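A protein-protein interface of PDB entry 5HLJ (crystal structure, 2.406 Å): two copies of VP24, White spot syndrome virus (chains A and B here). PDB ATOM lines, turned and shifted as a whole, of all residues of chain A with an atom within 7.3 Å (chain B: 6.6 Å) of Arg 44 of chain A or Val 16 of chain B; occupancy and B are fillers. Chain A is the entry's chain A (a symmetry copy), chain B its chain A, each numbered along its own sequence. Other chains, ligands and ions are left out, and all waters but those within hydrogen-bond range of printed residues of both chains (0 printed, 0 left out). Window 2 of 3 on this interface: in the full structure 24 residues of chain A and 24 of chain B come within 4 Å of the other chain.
OH of Tyr 46 of chain B lies within hydrogen-bond range of O of Glu 17 of chain B, 2.7 Å away. The guanidinium group (NH2) of Arg 167 of chain B sits at hydrogen-bond distance from the side-chain hydroxyl (OG) of Ser 18 of chain B. The backbone carbonyl oxygen of Glu 17 of chain A is in hydrogen-bond range of the side-chain hydroxyl of Tyr 46 of chain A, 2.7 Å away. OE2 of Glu 19 of chain A sits at hydrogen-bond distance from N of Arg 44 of chain A. The side-chain carboxylate of Glu 19 of chain A sits at hydrogen-bond distance from the backbone NH of Asn 45 of chain A, at 2.9 Å.
Printed residues of chain B within 4 Å of Ser 18 of chain A: Arg 167. Of the printed residues of chain B, Gln 42 of chain A touches Asp 173 (3.3 Å). Of chain A, only Arg 44 comes within 4 Å of Val 16 of chain B. Printed residues of chain A within 4 Å of Arg 167 of chain B: Ser 18, Glu 19 and Ile 20. The nearest residue of chain A that does not touch Val 16 of chain B is Glu 17 of chain A (4.8 Å). The nearest printed residue of chain B that does not touch Glu 17 of chain A is Val 16 of chain B (4.8 Å).
Glu 17 of chain A touches its own counterpart, Glu 17 of chain B. Of the 7 pairs that touch across the chains among the printed residues, 1 has its exchanged pair printed and touching as well.
The backbone carbonyl oxygen (O) of Val 16 of chain B sits at hydrogen-bond distance from the guanidinium group (NH2) of Arg 44 of chain A. The side-chain carboxylate (OE1) of Glu 17 of chain A lies close to the side-chain carboxylate (OE1) of Glu 17 of chain B (2.6 Å).
Hydrophobic or aromatic side chains of chain A within 4 Å of the printed part of chain B: Ile 20. Printed residues of chain B that touch a printed residue of chain A: Val 16, Glu 17, Arg 167, Pro 170 and Asp 173.
NH2 of Arg 167 of chain B touches O of Ser 18 of chain A, 3.8 Å away. Glu 19 of chain A touches Arg 167 of chain B. Ile 20 of chain A touches Arg 167 of chain B. O of Gln 42 of chain A touches CB of Asp 173 of chain B, at 3.3 Å. Arg 44 of chain A touches Pro 170 of chain B.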
ATOM      1  N   ALA A  13       2.630 -24.573   5.386  1.00  0.00           N
ATOM      2  CA  ALA A  13       1.311 -23.980   5.138  1.00  0.00           C
ATOM      3  C   ALA A  13       1.167 -22.549   5.684  1.00  0.00           C
ATOM      4  O   ALA A  13       1.512 -22.275   6.847  1.00  0.00           O
ATOM      5  CB  ALA A  13       0.216 -24.879   5.731  1.00  0.00           C
ATOM      6  N   PRO A  15      -1.951 -20.208   6.026  1.00  0.00           N
ATOM      7  CA  PRO A  15      -3.408 -20.068   5.870  1.00  0.00           C
ATOM      8  C   PRO A  15      -3.888 -18.625   5.798  1.00  0.00           C
ATOM      9  O   PRO A  15      -3.387 -17.762   6.525  1.00  0.00           O
ATOM     10  CB  PRO A  15      -3.956 -20.752   7.117  1.00  0.00           C
ATOM     11  CG  PRO A  15      -2.843 -20.669   8.133  1.00  0.00           C
ATOM     12  CD  PRO A  15      -1.574 -20.757   7.344  1.00  0.00           C
ATOM     13  N   GLU A  17      -7.534 -18.214   5.011  1.00  0.00           N
ATOM     14  CA  GLU A  17      -8.981 -18.351   5.218  1.00  0.00           C
ATOM     15  C   GLU A  17      -9.341 -19.311   6.343  1.00  0.00           C
ATOM     16  O   GLU A  17      -8.560 -20.197   6.696  1.00  0.00           O
ATOM     17  CB  GLU A  17      -9.675 -18.835   3.948  1.00  0.00           C
ATOM     18  CG  GLU A  17     -10.179 -17.735   3.046  1.00  0.00           C
ATOM     19  CD  GLU A  17      -9.649 -17.878   1.634  1.00  0.00           C
ATOM     20  OE1 GLU A  17      -9.779 -16.916   0.857  1.00  0.00           O
ATOM     21  OE2 GLU A  17      -9.096 -18.953   1.300  1.00  0.00           O
ATOM     22  N   SER A  18     -10.551 -19.149   6.866  1.00  0.00           N
ATOM     23  CA  SER A  18     -11.096 -20.046   7.869  1.00  0.00           C
ATOM     24  C   SER A  18     -11.476 -21.384   7.275  1.00  0.00           C
ATOM     25  O   SER A  18     -11.791 -21.473   6.103  1.00  0.00           O
ATOM     26  CB  SER A  18     -12.321 -19.435   8.527  1.00  0.00           C
ATOM     27  OG  SER A  18     -11.990 -18.195   9.108  1.00  0.00           O
ATOM     28  N   GLU A  19     -11.463 -22.421   8.100  1.00  0.00           N
ATOM     29  CA  GLU A  19     -11.875 -23.732   7.649  1.00  0.00           C
ATOM     30  C   GLU A  19     -12.409 -24.549   8.821  1.00  0.00           C
ATOM     31  O   GLU A  19     -11.994 -24.355   9.963  1.00  0.00           O
ATOM     32  CB  GLU A  19     -10.700 -24.434   6.964  1.00  0.00           C
ATOM     33  CG  GLU A  19     -11.054 -25.754   6.323  1.00  0.00           C
ATOM     34  CD  GLU A  19      -9.921 -26.328   5.491  1.00  0.00           C
ATOM     35  OE1 GLU A  19      -8.877 -25.645   5.331  1.00  0.00           O
ATOM     36  OE2 GLU A  19     -10.092 -27.458   4.981  1.00  0.00           O
ATOM     37  N   ILE A  20     -13.359 -25.434   8.539  1.00  0.00           N
ATOM     38  CA  ILE A  20     -13.882 -26.358   9.526  1.00  0.00           C
ATOM     39  C   ILE A  20     -13.124 -27.681   9.473  1.00  0.00           C
ATOM     40  O   ILE A  20     -12.904 -28.233   8.400  1.00  0.00           O
ATOM     41  CB  ILE A  20     -15.371 -26.622   9.303  1.00  0.00           C
ATOM     42  CG1 ILE A  20     -16.182 -25.349   9.527  1.00  0.00           C
ATOM     43  CG2 ILE A  20     -15.870 -27.654  10.261  1.00  0.00           C
ATOM     44  CD1 ILE A  20     -16.268 -24.938  10.953  1.00  0.00           C
ATOM     45  N   ILE A  21     -12.718 -28.164  10.644  1.00  0.00           N
ATOM     46  CA  ILE A  21     -12.002 -29.423  10.829  1.00  0.00           C
ATOM     47  C   ILE A  21     -12.970 -30.421  11.452  1.00  0.00           C
ATOM     48  O   ILE A  21     -13.435 -30.199  12.566  1.00  0.00           O
ATOM     49  CB  ILE A  21     -10.767 -29.236  11.765  1.00  0.00           C
ATOM     50  CG1 ILE A  21      -9.868 -28.092  11.270  1.00  0.00           C
ATOM     51  CG2 ILE A  21      -9.973 -30.513  11.920  1.00  0.00           C
ATOM     52  CD1 ILE A  21      -9.477 -28.201   9.810  1.00  0.00           C
ATOM     53  N   LEU A  41      -6.235 -35.933   8.233  1.00  0.00           N
ATOM     54  CA  LEU A  41      -7.205 -35.142   7.490  1.00  0.00           C
ATOM     55  C   LEU A  41      -6.456 -34.138   6.641  1.00  0.00           C
ATOM     56  O   LEU A  41      -5.674 -33.350   7.157  1.00  0.00           O
ATOM     57  CB  LEU A  41      -8.188 -34.426   8.431  1.00  0.00           C
ATOM     58  CG  LEU A  41      -9.120 -33.345   7.847  1.00  0.00           C
ATOM     59  CD1 LEU A  41     -10.141 -33.911   6.863  1.00  0.00           C
ATOM     60  CD2 LEU A  41      -9.834 -32.602   8.958  1.00  0.00           C
ATOM     61  N   GLN A  42      -6.677 -34.198   5.334  1.00  0.00           N
ATOM     62  CA  GLN A  42      -6.113 -33.219   4.425  1.00  0.00           C
ATOM     63  C   GLN A  42      -7.013 -31.980   4.374  1.00  0.00           C
ATOM     64  O   GLN A  42      -8.178 -32.065   4.010  1.00  0.00           O
ATOM     65  CB  GLN A  42      -5.944 -33.819   3.033  1.00  0.00           C
ATOM     66  CG  GLN A  42      -5.228 -32.891   2.078  1.00  0.00           C
ATOM     67  CD  GLN A  42      -3.824 -32.587   2.543  1.00  0.00           C
ATOM     68  OE1 GLN A  42      -3.057 -33.501   2.884  1.00  0.00           O
ATOM     69  NE2 GLN A  42      -3.478 -31.299   2.586  1.00  0.00           N
ATOM     70  N   THR A  43      -6.489 -30.832   4.775  1.00  0.00           N
ATOM     71  CA  THR A  43      -7.277 -29.607   4.725  1.00  0.00           C
ATOM     72  C   THR A  43      -6.872 -28.810   3.494  1.00  0.00           C
ATOM     73  O   THR A  43      -5.843 -29.105   2.877  1.00  0.00           O
ATOM     74  CB  THR A  43      -7.086 -28.750   5.997  1.00  0.00           C
ATOM     75  OG1 THR A  43      -5.798 -28.109   5.956  1.00  0.00           O
ATOM     76  CG2 THR A  43      -7.215 -29.618   7.253  1.00  0.00           C
ATOM     77  N   ARG A  44      -7.665 -27.801   3.139  1.00  0.00           N
ATOM     78  CA  ARG A  44      -7.301 -26.958   2.010  1.00  0.00           C
ATOM     79  C   ARG A  44      -6.370 -25.822   2.432  1.00  0.00           C
ATOM     80  O   ARG A  44      -5.528 -25.407   1.654  1.00  0.00           O
ATOM     81  CB  ARG A  44      -8.544 -26.383   1.305  1.00  0.00           C
ATOM     82  CG  ARG A  44      -9.792 -27.260   1.356  1.00  0.00           C
ATOM     83  CD  ARG A  44     -10.940 -26.698   0.472  1.00  0.00           C
ATOM     84  NE  ARG A  44     -10.881 -25.239   0.304  1.00  0.00           N
ATOM     85  CZ  ARG A  44     -11.435 -24.348   1.136  1.00  0.00           C
ATOM     86  NH1 ARG A  44     -12.097 -24.751   2.230  1.00  0.00           N
ATOM     87  NH2 ARG A  44     -11.315 -23.041   0.880  1.00  0.00           N
ATOM     88  N   ASN A  45      -6.511 -25.316   3.651  1.00  0.00           N
ATOM     89  CA  ASN A  45      -5.763 -24.130   4.045  1.00  0.00           C
ATOM     90  C   ASN A  45      -4.773 -24.356   5.185  1.00  0.00           C
ATOM     91  O   ASN A  45      -3.967 -23.478   5.472  1.00  0.00           O
ATOM     92  CB  ASN A  45      -6.728 -23.006   4.438  1.00  0.00           C
ATOM     93  CG  ASN A  45      -7.697 -22.642   3.320  1.00  0.00           C
ATOM     94  OD1 ASN A  45      -8.915 -22.669   3.504  1.00  0.00           O
ATOM     95  ND2 ASN A  45      -7.158 -22.292   2.160  1.00  0.00           N
ATOM     96  N   TYR A  46      -4.827 -25.515   5.837  1.00  0.00           N
ATOM     97  CA  TYR A  46      -4.030 -25.716   7.041  1.00  0.00           C
ATOM     98  C   TYR A  46      -3.089 -26.907   6.934  1.00  0.00           C
ATOM     99  O   TYR A  46      -2.600 -27.409   7.941  1.00  0.00           O
ATOM    100  CB  TYR A  46      -4.960 -25.844   8.263  1.00  0.00           C
ATOM    101  CG  TYR A  46      -5.642 -24.530   8.516  1.00  0.00           C
ATOM    102  CD1 TYR A  46      -5.040 -23.557   9.305  1.00  0.00           C
ATOM    103  CD2 TYR A  46      -6.841 -24.222   7.894  1.00  0.00           C
ATOM    104  CE1 TYR A  46      -5.636 -22.329   9.498  1.00  0.00           C
ATOM    105  CE2 TYR A  46      -7.443 -22.992   8.081  1.00  0.00           C
ATOM    106  CZ  TYR A  46      -6.836 -22.052   8.879  1.00  0.00           C
ATOM    107  OH  TYR A  46      -7.437 -20.832   9.060  1.00  0.00           O
ATOM    108  N   GLY A  47      -2.816 -27.344   5.711  1.00  0.00           N
ATOM    109  CA  GLY A  47      -1.934 -28.478   5.508  1.00  0.00           C
ATOM    110  C   GLY A  47      -2.580 -29.759   5.993  1.00  0.00           C
ATOM    111  O   GLY A  47      -3.813 -29.884   5.971  1.00  0.00           O
ATOM    112  N   TYR B  14     -17.771 -22.137  -9.736  1.00  0.00           N
ATOM    113  CA  TYR B  14     -16.565 -22.815  -9.249  1.00  0.00           C
ATOM    114  C   TYR B  14     -16.135 -22.263  -7.876  1.00  0.00           C
ATOM    115  O   TYR B  14     -15.282 -21.371  -7.798  1.00  0.00           O
ATOM    116  CB  TYR B  14     -15.416 -22.673 -10.259  1.00  0.00           C
ATOM    117  CG  TYR B  14     -14.219 -23.541  -9.939  1.00  0.00           C
ATOM    118  CD1 TYR B  14     -14.104 -24.821 -10.474  1.00  0.00           C
ATOM    119  CD2 TYR B  14     -13.211 -23.090  -9.089  1.00  0.00           C
ATOM    120  CE1 TYR B  14     -13.011 -25.625 -10.178  1.00  0.00           C
ATOM    121  CE2 TYR B  14     -12.119 -23.886  -8.785  1.00  0.00           C
ATOM    122  CZ  TYR B  14     -12.024 -25.149  -9.336  1.00  0.00           C
ATOM    123  OH  TYR B  14     -10.941 -25.947  -9.033  1.00  0.00           O
ATOM    124  N   PRO B  15     -16.713 -22.809  -6.789  1.00  0.00           N
ATOM    125  CA  PRO B  15     -16.512 -22.252  -5.442  1.00  0.00           C
ATOM    126  C   PRO B  15     -15.106 -22.454  -4.892  1.00  0.00           C
ATOM    127  O   PRO B  15     -14.508 -23.517  -5.078  1.00  0.00           O
ATOM    128  CB  PRO B  15     -17.529 -23.013  -4.598  1.00  0.00           C
ATOM    129  CG  PRO B  15     -17.770 -24.304  -5.342  1.00  0.00           C
ATOM    130  CD  PRO B  15     -17.636 -23.962  -6.793  1.00  0.00           C
ATOM    131  N   VAL B  16     -14.595 -21.442  -4.200  1.00  0.00           N
ATOM    132  CA  VAL B  16     -13.262 -21.532  -3.621  1.00  0.00           C
ATOM    133  C   VAL B  16     -13.264 -21.139  -2.136  1.00  0.00           C
ATOM    134  O   VAL B  16     -12.238 -21.232  -1.458  1.00  0.00           O
ATOM    135  CB  VAL B  16     -12.252 -20.659  -4.421  1.00  0.00           C
ATOM    136  CG1 VAL B  16     -11.870 -21.352  -5.736  1.00  0.00           C
ATOM    137  CG2 VAL B  16     -12.815 -19.263  -4.683  1.00  0.00           C
ATOM    138  N   GLU B  17     -14.426 -20.718  -1.635  1.00  0.00           N
ATOM    139  CA  GLU B  17     -14.597 -20.414  -0.209  1.00  0.00           C
ATOM    140  C   GLU B  17     -15.845 -21.042   0.397  1.00  0.00           C
ATOM    141  O   GLU B  17     -16.807 -21.351  -0.309  1.00  0.00           O
ATOM    142  CB  GLU B  17     -14.670 -18.907   0.026  1.00  0.00           C
ATOM    143  CG  GLU B  17     -13.343 -18.250   0.320  1.00  0.00           C
ATOM    144  CD  GLU B  17     -13.065 -17.097  -0.622  1.00  0.00           C
ATOM    145  OE1 GLU B  17     -11.913 -16.631  -0.656  1.00  0.00           O
ATOM    146  OE2 GLU B  17     -13.999 -16.658  -1.335  1.00  0.00           O
ATOM    147  N   SER B  18     -15.829 -21.184   1.717  1.00  0.00           N
ATOM    148  CA  SER B  18     -16.977 -21.662   2.467  1.00  0.00           C
ATOM    149  C   SER B  18     -18.070 -20.620   2.540  1.00  0.00           C
ATOM    150  O   SER B  18     -17.800 -19.434   2.477  1.00  0.00           O
ATOM    151  CB  SER B  18     -16.572 -22.050   3.878  1.00  0.00           C
ATOM    152  OG  SER B  18     -15.568 -23.037   3.840  1.00  0.00           O
ATOM    153  N   ASN B  45     -20.811 -17.760  -3.589  1.00  0.00           N
ATOM    154  CA  ASN B  45     -19.808 -18.693  -4.085  1.00  0.00           C
ATOM    155  C   ASN B  45     -20.378 -19.970  -4.698  1.00  0.00           C
ATOM    156  O   ASN B  45     -19.638 -20.734  -5.306  1.00  0.00           O
ATOM    157  CB  ASN B  45     -18.839 -19.071  -2.959  1.00  0.00           C
ATOM    158  CG  ASN B  45     -18.143 -17.860  -2.348  1.00  0.00           C
ATOM    159  OD1 ASN B  45     -18.207 -17.638  -1.137  1.00  0.00           O
ATOM    160  ND2 ASN B  45     -17.470 -17.081  -3.182  1.00  0.00           N
ATOM    161  N   TYR B  46     -21.679 -20.208  -4.543  1.00  0.00           N
ATOM    162  CA  TYR B  46     -22.242 -21.490  -4.951  1.00  0.00           C
ATOM    163  C   TYR B  46     -23.360 -21.344  -5.973  1.00  0.00           C
ATOM    164  O   TYR B  46     -24.147 -22.264  -6.173  1.00  0.00           O
ATOM    165  CB  TYR B  46     -22.716 -22.267  -3.708  1.00  0.00           C
ATOM    166  CG  TYR B  46     -21.528 -22.662  -2.878  1.00  0.00           C
ATOM    167  CD1 TYR B  46     -20.844 -23.844  -3.132  1.00  0.00           C
ATOM    168  CD2 TYR B  46     -21.030 -21.812  -1.903  1.00  0.00           C
ATOM    169  CE1 TYR B  46     -19.722 -24.186  -2.409  1.00  0.00           C
ATOM    170  CE2 TYR B  46     -19.904 -22.148  -1.175  1.00  0.00           C
ATOM    171  CZ  TYR B  46     -19.254 -23.331  -1.435  1.00  0.00           C
ATOM    172  OH  TYR B  46     -18.136 -23.658  -0.711  1.00  0.00           O
ATOM    173  N   ARG B 103     -17.658 -28.254  -8.986  1.00  0.00           N
ATOM    174  CA  ARG B 103     -16.870 -28.958  -7.973  1.00  0.00           C
ATOM    175  C   ARG B 103     -17.702 -29.692  -6.942  1.00  0.00           C
ATOM    176  O   ARG B 103     -18.847 -29.341  -6.681  1.00  0.00           O
ATOM    177  CB  ARG B 103     -15.940 -27.997  -7.243  1.00  0.00           C
ATOM    178  CG  ARG B 103     -14.630 -27.789  -7.948  1.00  0.00           C
ATOM    179  CD  ARG B 103     -13.628 -27.047  -7.081  1.00  0.00           C
ATOM    180  NE  ARG B 103     -13.390 -27.651  -5.770  1.00  0.00           N
ATOM    181  CZ  ARG B 103     -12.348 -27.335  -5.003  1.00  0.00           C
ATOM    182  NH1 ARG B 103     -11.475 -26.432  -5.421  1.00  0.00           N
ATOM    183  NH2 ARG B 103     -12.168 -27.917  -3.825  1.00  0.00           N
ATOM    184  N   ARG B 167     -23.419 -25.142   6.463  1.00  0.00           N
ATOM    185  CA  ARG B 167     -22.174 -24.619   5.936  1.00  0.00           C
ATOM    186  C   ARG B 167     -21.690 -25.446   4.758  1.00  0.00           C
ATOM    187  O   ARG B 167     -21.499 -26.651   4.873  1.00  0.00           O
ATOM    188  CB  ARG B 167     -21.089 -24.556   7.017  1.00  0.00           C
ATOM    189  CG  ARG B 167     -19.780 -23.983   6.468  1.00  0.00           C
ATOM    190  CD  ARG B 167     -18.724 -23.763   7.550  1.00  0.00           C
ATOM    191  NE  ARG B 167     -17.370 -23.688   6.987  1.00  0.00           N
ATOM    192  CZ  ARG B 167     -16.485 -22.729   7.277  1.00  0.00           C
ATOM    193  NH1 ARG B 167     -16.812 -21.742   8.119  1.00  0.00           N
ATOM    194  NH2 ARG B 167     -15.267 -22.751   6.729  1.00  0.00           N
ATOM    195  N   SER B 169     -18.655 -26.044   1.906  1.00  0.00           N
ATOM    196  CA  SER B 169     -17.256 -25.769   1.597  1.00  0.00           C
ATOM    197  C   SER B 169     -16.798 -26.575   0.378  1.00  0.00           C
ATOM    198  O   SER B 169     -17.389 -27.598   0.049  1.00  0.00           O
ATOM    199  CB  SER B 169     -16.372 -26.046   2.827  1.00  0.00           C
ATOM    200  OG  SER B 169     -16.490 -27.385   3.252  1.00  0.00           O
ATOM    201  N   PRO B 170     -15.755 -26.098  -0.313  1.00  0.00           N
ATOM    202  CA  PRO B 170     -15.311 -26.783  -1.530  1.00  0.00           C
ATOM    203  C   PRO B 170     -14.622 -28.103  -1.249  1.00  0.00           C
ATOM    204  O   PRO B 170     -13.942 -28.230  -0.237  1.00  0.00           O
ATOM    205  CB  PRO B 170     -14.314 -25.790  -2.153  1.00  0.00           C
ATOM    206  CG  PRO B 170     -14.520 -24.497  -1.423  1.00  0.00           C
ATOM    207  CD  PRO B 170     -14.982 -24.867  -0.064  1.00  0.00           C
ATOM    208  N   GLY B 171     -14.785 -29.073  -2.142  1.00  0.00           N
ATOM    209  CA  GLY B 171     -13.966 -30.268  -2.088  1.00  0.00           C
ATOM    210  C   GLY B 171     -14.661 -31.410  -1.384  1.00  0.00           C
ATOM    211  O   GLY B 171     -15.853 -31.333  -1.057  1.00  0.00           O
ATOM    212  N   ASP B 173     -12.582 -33.722   0.857  1.00  0.00           N
ATOM    213  CA  ASP B 173     -11.672 -34.296   1.852  1.00  0.00           C
ATOM    214  C   ASP B 173     -12.351 -34.522   3.199  1.00  0.00           C
ATOM    215  O   ASP B 173     -12.989 -33.622   3.753  1.00  0.00           O
ATOM    216  CB  ASP B 173     -10.440 -33.401   2.050  1.00  0.00           C
ATOM    217  CG  ASP B 173      -9.450 -33.502   0.904  1.00  0.00           C
ATOM    218  OD1 ASP B 173      -9.104 -34.639   0.503  1.00  0.00           O
ATOM    219  OD2 ASP B 173      -9.019 -32.435   0.407  1.00  0.00           O
